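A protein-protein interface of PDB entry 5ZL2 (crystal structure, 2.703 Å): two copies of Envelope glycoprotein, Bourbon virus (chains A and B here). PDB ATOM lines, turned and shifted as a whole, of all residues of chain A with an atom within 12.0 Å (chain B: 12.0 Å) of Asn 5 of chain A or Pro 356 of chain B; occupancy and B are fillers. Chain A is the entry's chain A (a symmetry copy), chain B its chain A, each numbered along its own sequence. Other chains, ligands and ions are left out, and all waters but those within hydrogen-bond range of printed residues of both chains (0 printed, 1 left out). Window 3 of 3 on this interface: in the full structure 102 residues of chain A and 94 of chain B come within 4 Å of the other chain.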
ATOM      1  N   LEU A   3      34.371  15.406  -7.247  1.00  0.00           N
ATOM      2  CA  LEU A   3      33.581  14.819  -6.175  1.00  0.00           C
ATOM      3  C   LEU A   3      33.184  15.854  -5.127  1.00  0.00           C
ATOM      4  O   LEU A   3      33.828  16.896  -4.975  1.00  0.00           O
ATOM      5  CB  LEU A   3      34.350  13.676  -5.509  1.00  0.00           C
ATOM      6  CG  LEU A   3      33.530  12.714  -4.647  1.00  0.00           C
ATOM      7  CD1 LEU A   3      32.781  11.727  -5.528  1.00  0.00           C
ATOM      8  CD2 LEU A   3      34.402  11.989  -3.630  1.00  0.00           C
ATOM      9  N   CYS A   4      32.116  15.540  -4.398  1.00  0.00           N
ATOM     10  CA  CYS A   4      31.593  16.416  -3.362  1.00  0.00           C
ATOM     11  C   CYS A   4      31.395  15.643  -2.057  1.00  0.00           C
ATOM     12  O   CYS A   4      31.817  14.488  -1.950  1.00  0.00           O
ATOM     13  CB  CYS A   4      30.302  17.068  -3.853  1.00  0.00           C
ATOM     14  SG  CYS A   4      30.418  17.880  -5.476  1.00  0.00           S
ATOM     15  N   ASN A   5      30.754  16.259  -1.063  1.00  0.00           N
ATOM     16  CA  ASN A   5      30.833  15.806   0.330  1.00  0.00           C
ATOM     17  C   ASN A   5      29.432  15.626   0.927  1.00  0.00           C
ATOM     18  O   ASN A   5      29.104  16.191   1.971  1.00  0.00           O
ATOM     19  CB  ASN A   5      31.658  16.767   1.186  1.00  0.00           C
ATOM     20  CG  ASN A   5      32.150  16.121   2.470  1.00  0.00           C
ATOM     21  OD1 ASN A   5      32.045  14.908   2.641  1.00  0.00           O
ATOM     22  ND2 ASN A   5      32.695  16.928   3.372  1.00  0.00           N
ATOM     23  N   LYS A   6      28.602  14.823   0.251  1.00  0.00           N
ATOM     24  CA  LYS A   6      27.187  14.625   0.571  1.00  0.00           C
ATOM     25  C   LYS A   6      26.886  14.490   2.060  1.00  0.00           C
ATOM     26  O   LYS A   6      25.751  14.725   2.490  1.00  0.00           O
ATOM     27  CB  LYS A   6      26.660  13.363  -0.121  1.00  0.00           C
ATOM     28  CG  LYS A   6      26.745  13.297  -1.644  1.00  0.00           C
ATOM     29  CD  LYS A   6      26.343  14.603  -2.285  1.00  0.00           C
ATOM     30  CE  LYS A   6      27.545  15.369  -2.789  1.00  0.00           C
ATOM     31  NZ  LYS A   6      27.258  16.825  -2.752  1.00  0.00           N
ATOM     32  N   GLN A   7      27.890  14.072   2.836  1.00  0.00           N
ATOM     33  CA  GLN A   7      27.733  13.802   4.260  1.00  0.00           C
ATOM     34  C   GLN A   7      26.918  14.871   4.981  1.00  0.00           C
ATOM     35  O   GLN A   7      25.838  14.592   5.514  1.00  0.00           O
ATOM     36  CB  GLN A   7      29.119  13.666   4.901  1.00  0.00           C
ATOM     37  CG  GLN A   7      29.767  12.314   4.679  1.00  0.00           C
ATOM     38  CD  GLN A   7      29.051  11.210   5.427  1.00  0.00           C
ATOM     39  OE1 GLN A   7      28.606  11.400   6.559  1.00  0.00           O
ATOM     40  NE2 GLN A   7      28.925  10.048   4.794  1.00  0.00           N
ATOM     41  N   GLN A   8      27.412  16.105   4.986  1.00  0.00           N
ATOM     42  CA  GLN A   8      26.809  17.164   5.780  1.00  0.00           C
ATOM     43  C   GLN A   8      26.438  18.357   4.910  1.00  0.00           C
ATOM     44  O   GLN A   8      27.088  18.650   3.900  1.00  0.00           O
ATOM     45  CB  GLN A   8      27.736  17.592   6.912  1.00  0.00           C
ATOM     46  CG  GLN A   8      28.209  16.418   7.750  1.00  0.00           C
ATOM     47  CD  GLN A   8      27.078  15.593   8.330  1.00  0.00           C
ATOM     48  OE1 GLN A   8      26.028  16.122   8.694  1.00  0.00           O
ATOM     49  NE2 GLN A   8      27.292  14.285   8.429  1.00  0.00           N
ATOM     50  N   GLN A   9      25.380  19.039   5.326  1.00  0.00           N
ATOM     51  CA  GLN A   9      24.654  20.006   4.520  1.00  0.00           C
ATOM     52  C   GLN A   9      24.636  21.362   5.231  1.00  0.00           C
ATOM     53  O   GLN A   9      25.340  21.578   6.221  1.00  0.00           O
ATOM     54  CB  GLN A   9      23.242  19.483   4.247  1.00  0.00           C
ATOM     55  CG  GLN A   9      23.119  18.587   3.013  1.00  0.00           C
ATOM     56  CD  GLN A   9      23.346  17.108   3.296  1.00  0.00           C
ATOM     57  OE1 GLN A   9      24.160  16.735   4.137  1.00  0.00           O
ATOM     58  NE2 GLN A   9      22.609  16.257   2.591  1.00  0.00           N
ATOM     59  N   GLN A  10      23.841  22.289   4.699  1.00  0.00           N
ATOM     60  CA  GLN A  10      23.636  23.575   5.352  1.00  0.00           C
ATOM     61  C   GLN A  10      22.304  24.157   4.903  1.00  0.00           C
ATOM     62  O   GLN A  10      21.966  24.104   3.719  1.00  0.00           O
ATOM     63  CB  GLN A  10      24.767  24.565   5.047  1.00  0.00           C
ATOM     64  CG  GLN A  10      25.002  25.603   6.146  1.00  0.00           C
ATOM     65  CD  GLN A  10      23.869  26.607   6.281  1.00  0.00           C
ATOM     66  OE1 GLN A  10      23.210  26.954   5.301  1.00  0.00           O
ATOM     67  NE2 GLN A  10      23.636  27.075   7.503  1.00  0.00           N
ATOM     68  N   GLY A  11      21.566  24.719   5.855  1.00  0.00           N
ATOM     69  CA  GLY A  11      20.316  25.376   5.567  1.00  0.00           C
ATOM     70  C   GLY A  11      19.272  25.118   6.633  1.00  0.00           C
ATOM     71  O   GLY A  11      19.543  25.217   7.834  1.00  0.00           O
ATOM     72  N   PHE A  13      17.573  26.120   2.838  1.00  0.00           N
ATOM     73  CA  PHE A  13      17.487  27.364   2.089  1.00  0.00           C
ATOM     74  C   PHE A  13      16.164  27.446   1.340  1.00  0.00           C
ATOM     75  O   PHE A  13      15.449  26.457   1.169  1.00  0.00           O
ATOM     76  CB  PHE A  13      18.647  27.485   1.095  1.00  0.00           C
ATOM     77  CG  PHE A  13      19.932  27.942   1.711  1.00  0.00           C
ATOM     78  CD1 PHE A  13      20.088  29.248   2.133  1.00  0.00           C
ATOM     79  CD2 PHE A  13      20.995  27.067   1.850  1.00  0.00           C
ATOM     80  CE1 PHE A  13      21.280  29.670   2.694  1.00  0.00           C
ATOM     81  CE2 PHE A  13      22.185  27.485   2.408  1.00  0.00           C
ATOM     82  CZ  PHE A  13      22.328  28.788   2.831  1.00  0.00           C
ATOM     83  N   ASP B 331      21.896  18.177  -9.336  1.00  0.00           N
ATOM     84  CA  ASP B 331      22.369  18.803  -8.108  1.00  0.00           C
ATOM     85  C   ASP B 331      23.533  19.755  -8.348  1.00  0.00           C
ATOM     86  O   ASP B 331      23.915  20.484  -7.426  1.00  0.00           O
ATOM     87  CB  ASP B 331      22.769  17.737  -7.086  1.00  0.00           C
ATOM     88  CG  ASP B 331      23.758  16.729  -7.645  1.00  0.00           C
ATOM     89  OD1 ASP B 331      24.045  16.782  -8.861  1.00  0.00           O
ATOM     90  OD2 ASP B 331      24.251  15.887  -6.866  1.00  0.00           O
ATOM     91  N   ARG B 332      24.105  19.766  -9.548  1.00  0.00           N
ATOM     92  CA  ARG B 332      25.169  20.699  -9.885  1.00  0.00           C
ATOM     93  C   ARG B 332      24.646  22.007 -10.445  1.00  0.00           C
ATOM     94  O   ARG B 332      25.446  22.874 -10.811  1.00  0.00           O
ATOM     95  CB  ARG B 332      26.131  20.076 -10.899  1.00  0.00           C
ATOM     96  CG  ARG B 332      26.911  18.847 -10.427  1.00  0.00           C
ATOM     97  CD  ARG B 332      27.082  18.724  -8.907  1.00  0.00           C
ATOM     98  NE  ARG B 332      27.599  19.930  -8.269  1.00  0.00           N
ATOM     99  CZ  ARG B 332      28.854  20.352  -8.360  1.00  0.00           C
ATOM    100  NH1 ARG B 332      29.737  19.670  -9.073  1.00  0.00           N
ATOM    101  NH2 ARG B 332      29.227  21.462  -7.737  1.00  0.00           N
ATOM    102  N   LEU B 333      23.328  22.168 -10.529  1.00  0.00           N
ATOM    103  CA  LEU B 333      22.772  23.352 -11.170  1.00  0.00           C
ATOM    104  C   LEU B 333      22.949  24.588 -10.300  1.00  0.00           C
ATOM    105  O   LEU B 333      23.605  25.555 -10.701  1.00  0.00           O
ATOM    106  CB  LEU B 333      21.295  23.139 -11.478  1.00  0.00           C
ATOM    107  CG  LEU B 333      20.677  24.405 -12.064  1.00  0.00           C
ATOM    108  CD1 LEU B 333      21.258  24.708 -13.439  1.00  0.00           C
ATOM    109  CD2 LEU B 333      19.172  24.300 -12.092  1.00  0.00           C
ATOM    110  N   ILE B 334      22.350  24.576  -9.105  1.00  0.00           N
ATOM    111  CA  ILE B 334      22.334  25.762  -8.253  1.00  0.00           C
ATOM    112  C   ILE B 334      23.749  26.265  -8.014  1.00  0.00           C
ATOM    113  O   ILE B 334      23.993  27.476  -7.935  1.00  0.00           O
ATOM    114  CB  ILE B 334      21.603  25.453  -6.931  1.00  0.00           C
ATOM    115  CG1 ILE B 334      20.113  25.221  -7.189  1.00  0.00           C
ATOM    116  CG2 ILE B 334      21.799  26.574  -5.917  1.00  0.00           C
ATOM    117  CD1 ILE B 334      19.333  24.856  -5.944  1.00  0.00           C
ATOM    118  N   GLY B 335      24.708  25.348  -7.920  1.00  0.00           N
ATOM    119  CA  GLY B 335      26.091  25.766  -7.789  1.00  0.00           C
ATOM    120  C   GLY B 335      26.585  26.530  -9.001  1.00  0.00           C
ATOM    121  O   GLY B 335      27.343  27.494  -8.873  1.00  0.00           O
ATOM    122  N   ALA B 336      26.159  26.111 -10.195  1.00  0.00           N
ATOM    123  CA  ALA B 336      26.531  26.834 -11.407  1.00  0.00           C
ATOM    124  C   ALA B 336      25.846  28.192 -11.467  1.00  0.00           C
ATOM    125  O   ALA B 336      26.448  29.181 -11.901  1.00  0.00           O
ATOM    126  CB  ALA B 336      26.183  26.005 -12.641  1.00  0.00           C
ATOM    127  N   LEU B 338      25.074  30.027  -8.970  1.00  0.00           N
ATOM    128  CA  LEU B 338      25.775  30.876  -8.019  1.00  0.00           C
ATOM    129  C   LEU B 338      27.270  30.938  -8.286  1.00  0.00           C
ATOM    130  O   LEU B 338      27.989  31.610  -7.540  1.00  0.00           O
ATOM    131  CB  LEU B 338      25.523  30.386  -6.592  1.00  0.00           C
ATOM    132  CG  LEU B 338      24.055  30.424  -6.175  1.00  0.00           C
ATOM    133  CD1 LEU B 338      23.876  29.859  -4.780  1.00  0.00           C
ATOM    134  CD2 LEU B 338      23.532  31.847  -6.254  1.00  0.00           C
ATOM    135  N   GLU B 339      27.747  30.255  -9.327  1.00  0.00           N
ATOM    136  CA  GLU B 339      29.166  30.232  -9.684  1.00  0.00           C
ATOM    137  C   GLU B 339      30.034  29.755  -8.521  1.00  0.00           C
ATOM    138  O   GLU B 339      31.212  30.108  -8.424  1.00  0.00           O
ATOM    139  CB  GLU B 339      29.629  31.602 -10.193  1.00  0.00           C
ATOM    140  CG  GLU B 339      28.920  32.033 -11.478  1.00  0.00           C
ATOM    141  CD  GLU B 339      29.202  33.476 -11.867  1.00  0.00           C
ATOM    142  OE1 GLU B 339      28.765  34.390 -11.135  1.00  0.00           O
ATOM    143  OE2 GLU B 339      29.855  33.694 -12.910  1.00  0.00           O
ATOM    144  N   LYS B 340      29.452  28.946  -7.633  1.00  0.00           N
ATOM    145  CA  LYS B 340      30.135  28.312  -6.521  1.00  0.00           C
ATOM    146  C   LYS B 340      30.065  26.796  -6.663  1.00  0.00           C
ATOM    147  O   LYS B 340      29.015  26.261  -7.031  1.00  0.00           O
ATOM    148  CB  LYS B 340      29.514  28.717  -5.176  1.00  0.00           C
ATOM    149  CG  LYS B 340      30.154  29.926  -4.521  1.00  0.00           C
ATOM    150  CD  LYS B 340      29.443  30.275  -3.220  1.00  0.00           C
ATOM    151  CE  LYS B 340      27.963  30.530  -3.452  1.00  0.00           C
ATOM    152  NZ  LYS B 340      27.413  31.501  -2.467  1.00  0.00           N
ATOM    153  N   PRO B 341      31.155  26.079  -6.390  1.00  0.00           N
ATOM    154  CA  PRO B 341      31.097  24.612  -6.450  1.00  0.00           C
ATOM    155  C   PRO B 341      30.322  24.019  -5.281  1.00  0.00           C
ATOM    156  O   PRO B 341      30.789  24.046  -4.137  1.00  0.00           O
ATOM    157  CB  PRO B 341      32.576  24.204  -6.421  1.00  0.00           C
ATOM    158  CG  PRO B 341      33.257  25.328  -5.712  1.00  0.00           C
ATOM    159  CD  PRO B 341      32.511  26.574  -6.098  1.00  0.00           C
ATOM    160  N   MET B 342      29.136  23.480  -5.554  1.00  0.00           N
ATOM    161  CA  MET B 342      28.289  22.951  -4.494  1.00  0.00           C
ATOM    162  C   MET B 342      27.264  22.007  -5.103  1.00  0.00           C
ATOM    163  O   MET B 342      27.012  22.030  -6.311  1.00  0.00           O
ATOM    164  CB  MET B 342      27.587  24.073  -3.723  1.00  0.00           C
ATOM    165  CG  MET B 342      26.417  24.688  -4.473  1.00  0.00           C
ATOM    166  SD  MET B 342      25.404  25.788  -3.468  1.00  0.00           S
ATOM    167  CE  MET B 342      26.619  27.003  -2.970  1.00  0.00           C
ATOM    168  N   ALA B 343      26.668  21.177  -4.251  1.00  0.00           N
ATOM    169  CA  ALA B 343      25.641  20.240  -4.681  1.00  0.00           C
ATOM    170  C   ALA B 343      24.409  20.388  -3.804  1.00  0.00           C
ATOM    171  O   ALA B 343      24.517  20.604  -2.593  1.00  0.00           O
ATOM    172  CB  ALA B 343      26.138  18.797  -4.640  1.00  0.00           C
ATOM    173  N   SER B 344      23.244  20.250  -4.424  1.00  0.00           N
ATOM    174  CA  SER B 344      21.969  20.567  -3.803  1.00  0.00           C
ATOM    175  C   SER B 344      21.262  19.308  -3.314  1.00  0.00           C
ATOM    176  O   SER B 344      21.336  18.243  -3.934  1.00  0.00           O
ATOM    177  CB  SER B 344      21.069  21.315  -4.787  1.00  0.00           C
ATOM    178  OG  SER B 344      20.750  20.500  -5.903  1.00  0.00           O
ATOM    179  N   LYS B 345      20.552  19.456  -2.198  1.00  0.00           N
ATOM    180  CA  LYS B 345      19.864  18.355  -1.528  1.00  0.00           C
ATOM    181  C   LYS B 345      18.569  18.914  -0.963  1.00  0.00           C
ATOM    182  O   LYS B 345      18.602  19.702  -0.013  1.00  0.00           O
ATOM    183  CB  LYS B 345      20.736  17.767  -0.417  1.00  0.00           C
ATOM    184  CG  LYS B 345      20.255  16.458   0.209  1.00  0.00           C
ATOM    185  CD  LYS B 345      19.681  15.468  -0.795  1.00  0.00           C
ATOM    186  CE  LYS B 345      19.520  14.087  -0.150  1.00  0.00           C
ATOM    187  NZ  LYS B 345      18.326  13.345  -0.640  1.00  0.00           N
ATOM    188  N   PHE B 352      15.912  23.346   0.349  1.00  0.00           N
ATOM    189  CA  PHE B 352      17.005  22.452   0.019  1.00  0.00           C
ATOM    190  C   PHE B 352      18.181  22.718   0.947  1.00  0.00           C
ATOM    191  O   PHE B 352      18.175  23.654   1.757  1.00  0.00           O
ATOM    192  CB  PHE B 352      17.426  22.593  -1.450  1.00  0.00           C
ATOM    193  CG  PHE B 352      17.851  23.979  -1.831  1.00  0.00           C
ATOM    194  CD1 PHE B 352      16.949  24.870  -2.386  1.00  0.00           C
ATOM    195  CD2 PHE B 352      19.156  24.390  -1.642  1.00  0.00           C
ATOM    196  CE1 PHE B 352      17.340  26.145  -2.740  1.00  0.00           C
ATOM    197  CE2 PHE B 352      19.554  25.663  -1.993  1.00  0.00           C
ATOM    198  CZ  PHE B 352      18.646  26.540  -2.541  1.00  0.00           C
ATOM    199  N   MET B 353      19.197  21.874   0.803  1.00  0.00           N
ATOM    200  CA  MET B 353      20.424  21.927   1.573  1.00  0.00           C
ATOM    201  C   MET B 353      21.598  21.926   0.606  1.00  0.00           C
ATOM    202  O   MET B 353      21.529  21.333  -0.473  1.00  0.00           O
ATOM    203  CB  MET B 353      20.508  20.728   2.522  1.00  0.00           C
ATOM    204  CG  MET B 353      19.406  20.659   3.558  1.00  0.00           C
ATOM    205  SD  MET B 353      19.773  21.707   4.972  1.00  0.00           S
ATOM    206  CE  MET B 353      18.435  21.253   6.068  1.00  0.00           C
ATOM    207  N   VAL B 354      22.672  22.607   0.984  1.00  0.00           N
ATOM    208  CA  VAL B 354      23.821  22.795   0.107  1.00  0.00           C
ATOM    209  C   VAL B 354      25.047  22.166   0.760  1.00  0.00           C
ATOM    210  O   VAL B 354      25.259  22.302   1.969  1.00  0.00           O
ATOM    211  CB  VAL B 354      24.047  24.284  -0.229  1.00  0.00           C
ATOM    212  CG1 VAL B 354      22.845  24.828  -0.985  1.00  0.00           C
ATOM    213  CG2 VAL B 354      24.308  25.127   1.022  1.00  0.00           C
ATOM    214  N   SER B 355      25.832  21.456  -0.039  1.00  0.00           N
ATOM    215  CA  SER B 355      27.006  20.709   0.376  1.00  0.00           C
ATOM    216  C   SER B 355      28.176  21.093  -0.517  1.00  0.00           C
ATOM    217  O   SER B 355      27.977  21.443  -1.682  1.00  0.00           O
ATOM    218  CB  SER B 355      26.749  19.193   0.288  1.00  0.00           C
ATOM    219  OG  SER B 355      25.576  18.815   0.992  1.00  0.00           O
ATOM    220  N   PRO B 356      29.400  21.047  -0.002  1.00  0.00           N
ATOM    221  CA  PRO B 356      30.546  21.569  -0.758  1.00  0.00           C
ATOM    222  C   PRO B 356      30.868  20.729  -1.984  1.00  0.00           C
ATOM    223  O   PRO B 356      30.327  19.646  -2.200  1.00  0.00           O
ATOM    224  CB  PRO B 356      31.690  21.511   0.254  1.00  0.00           C
ATOM    225  CG  PRO B 356      31.273  20.473   1.240  1.00  0.00           C
ATOM    226  CD  PRO B 356      29.787  20.602   1.347  1.00  0.00           C
ATOM    227  N   CYS B 357      31.783  21.261  -2.791  1.00  0.00           N
ATOM    228  CA  CYS B 357      32.356  20.557  -3.935  1.00  0.00           C
ATOM    229  C   CYS B 357      33.769  21.080  -4.176  1.00  0.00           C
ATOM    230  O   CYS B 357      34.498  20.582  -5.029  1.00  0.00           O
ATOM    231  CB  CYS B 357      31.502  20.739  -5.193  1.00  0.00           C
ATOM    232  SG  CYS B 357      29.938  19.836  -5.206  1.00  0.00           S
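No position is printed for both chains. Of the 16 pairs that touch across the chains among the printed residues, none has its exchanged pair printed and touching as well.
Of the printed residues of chain B, Asn 5 of chain A touches Pro 356 (3.6 Å). Pro 356 of chain B touches just these residues of chain A: Cys 4 (3.1 Å) and Asn 5 (3.6 Å). Of chain B, only Cys 357 comes within 4 Å of Leu 3 of chain A. Cys 4 of chain A touches just these residues of chain B: Pro 356 and Cys 357. Lys 6 of chain A touches two residues of chain B. Of chain B, only Ser 355 comes within 4 Å of Gln 8 of chain A. Of chain B, only Lys 345, Met 353, Val 354 and Ser 355 come within 4 Å of Gln 9 of chain A. Pro 341 of chain B touches none of the printed residues of chain A. No residue of chain A comes within 4 Å of Met 342 of chain B. Of chain A, only Lys 6 (3.9 Å), Gln 8 (3.3 Å) and Gln 9 (3.2 Å) come within 4 Å of Ser 355 of chain B. Printed residues of chain B within 4 Å of Gly 11 of chain A: Met 353. Of the printed residues of chain A, Lys 345 of chain B touches Gln 9 (3.4 Å). Of the printed residues of chain A, Phe 352 of chain B touches Phe 13. Of the printed residues of chain B, Gln 10 of chain A touches Met 353 and Val 354. Arg 332 of chain B touches none of the printed residues of chain A. The nearest printed residue of chain A that does not touch Pro 356 of chain B is Gln 8 of chain A (4.2 Å). The nearest printed residue of chain B that does not touch Phe 13 of chain A is Met 353 of chain B (5.0 Å).
The backbone carbonyl oxygen of Phe 352 of chain B sits at hydrogen-bond distance from the backbone NH of Phe 13 of chain A. SD of Met 353 of chain B sits at hydrogen-bond distance from N of Gly 11 of chain A (3.6 Å). The backbone carbonyl oxygen (O) of Val 354 of chain B sits at hydrogen-bond distance from the backbone NH (N) of Gln 10 of chain A, 3.1 Å away. OG of Ser 355 of chain B is in hydrogen-bond range of O of Gln 8 of chain A (3.3 Å). The side-chain sulfur (SG) of Cys 357 of chain B forms a disulfide with the side-chain sulfur (SG) of Cys 4 of chain A (2.0 Å). The side-chain sulfur of Cys 4 of chain A lies close to the backbone carbonyl oxygen of Pro 356 of chain B, at 3.7 Å. SD of Met 353 of chain B sits close to O of Gln 10 of chain A (3.5 Å).
The guanidinium group (NH2) of Arg 332 of chain B lies within hydrogen-bond range of the side-chain sulfur (SG) of Cys 357 of chain B (3.1 Å). The backbone carbonyl oxygen (O) of Pro 341 of chain B lies within hydrogen-bond range of the backbone NH (N) of Cys 357 of chain B (3.2 Å). SG of Cys 357 of chain B sits close to N of Met 342 of chain B. SG of Cys 357 of chain B sits at hydrogen-bond distance from N of Ala 343 of chain B. The backbone carbonyl oxygen (O) of Met 353 of chain B sits at hydrogen-bond distance from the backbone NH (N) of Lys 345 of chain B (2.7 Å). O of Gln 7 of chain A lies close to OE1 of Gln 9 of chain A (3.1 Å).
Among the printed residues, pairs that only touch across the chains: Leu 3 of chain A with Cys 357 of chain B (3.7 Å), Asn 5 of chain A with Pro 356 of chain B (3.6 Å), Lys 6 of chain A with Ala 343 of chain B (3.0 Å), Lys 6 of chain A with Ser 355 of chain B (3.9 Å), Gln 9 of chain A with Lys 345 of chain B (3.4 Å), Gln 9 of chain A with Met 353 of chain B (3.4 Å), Gln 9 of chain A with Val 354 of chain B (3.5 Å), Gln 9 of chain A with Ser 355 of chain B (3.2 Å) and Phe 13 of chain A with Val 354 of chain B (3.5 Å).
Of the 10 printed residues of chain A, 9 touch a printed residue of chain B. Hydrophobic or aromatic side chains of chain A that line the printed part of chain B: Phe 13. Along chain A the printed residues that touch a printed residue of chain B span positions 3 to 13. Hydrophobic or aromatic side chains of chain B within 4 Å of the printed part of chain A: Ala 343, Phe 352, Met 353, Val 354 and Pro 356. Among the printed residues, 16 pairs touch across the chains. Among the printed residues, no Asp or Glu carboxylate lies within 4 Å of a Lys or Arg side-chain nitrogen of the other chain.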
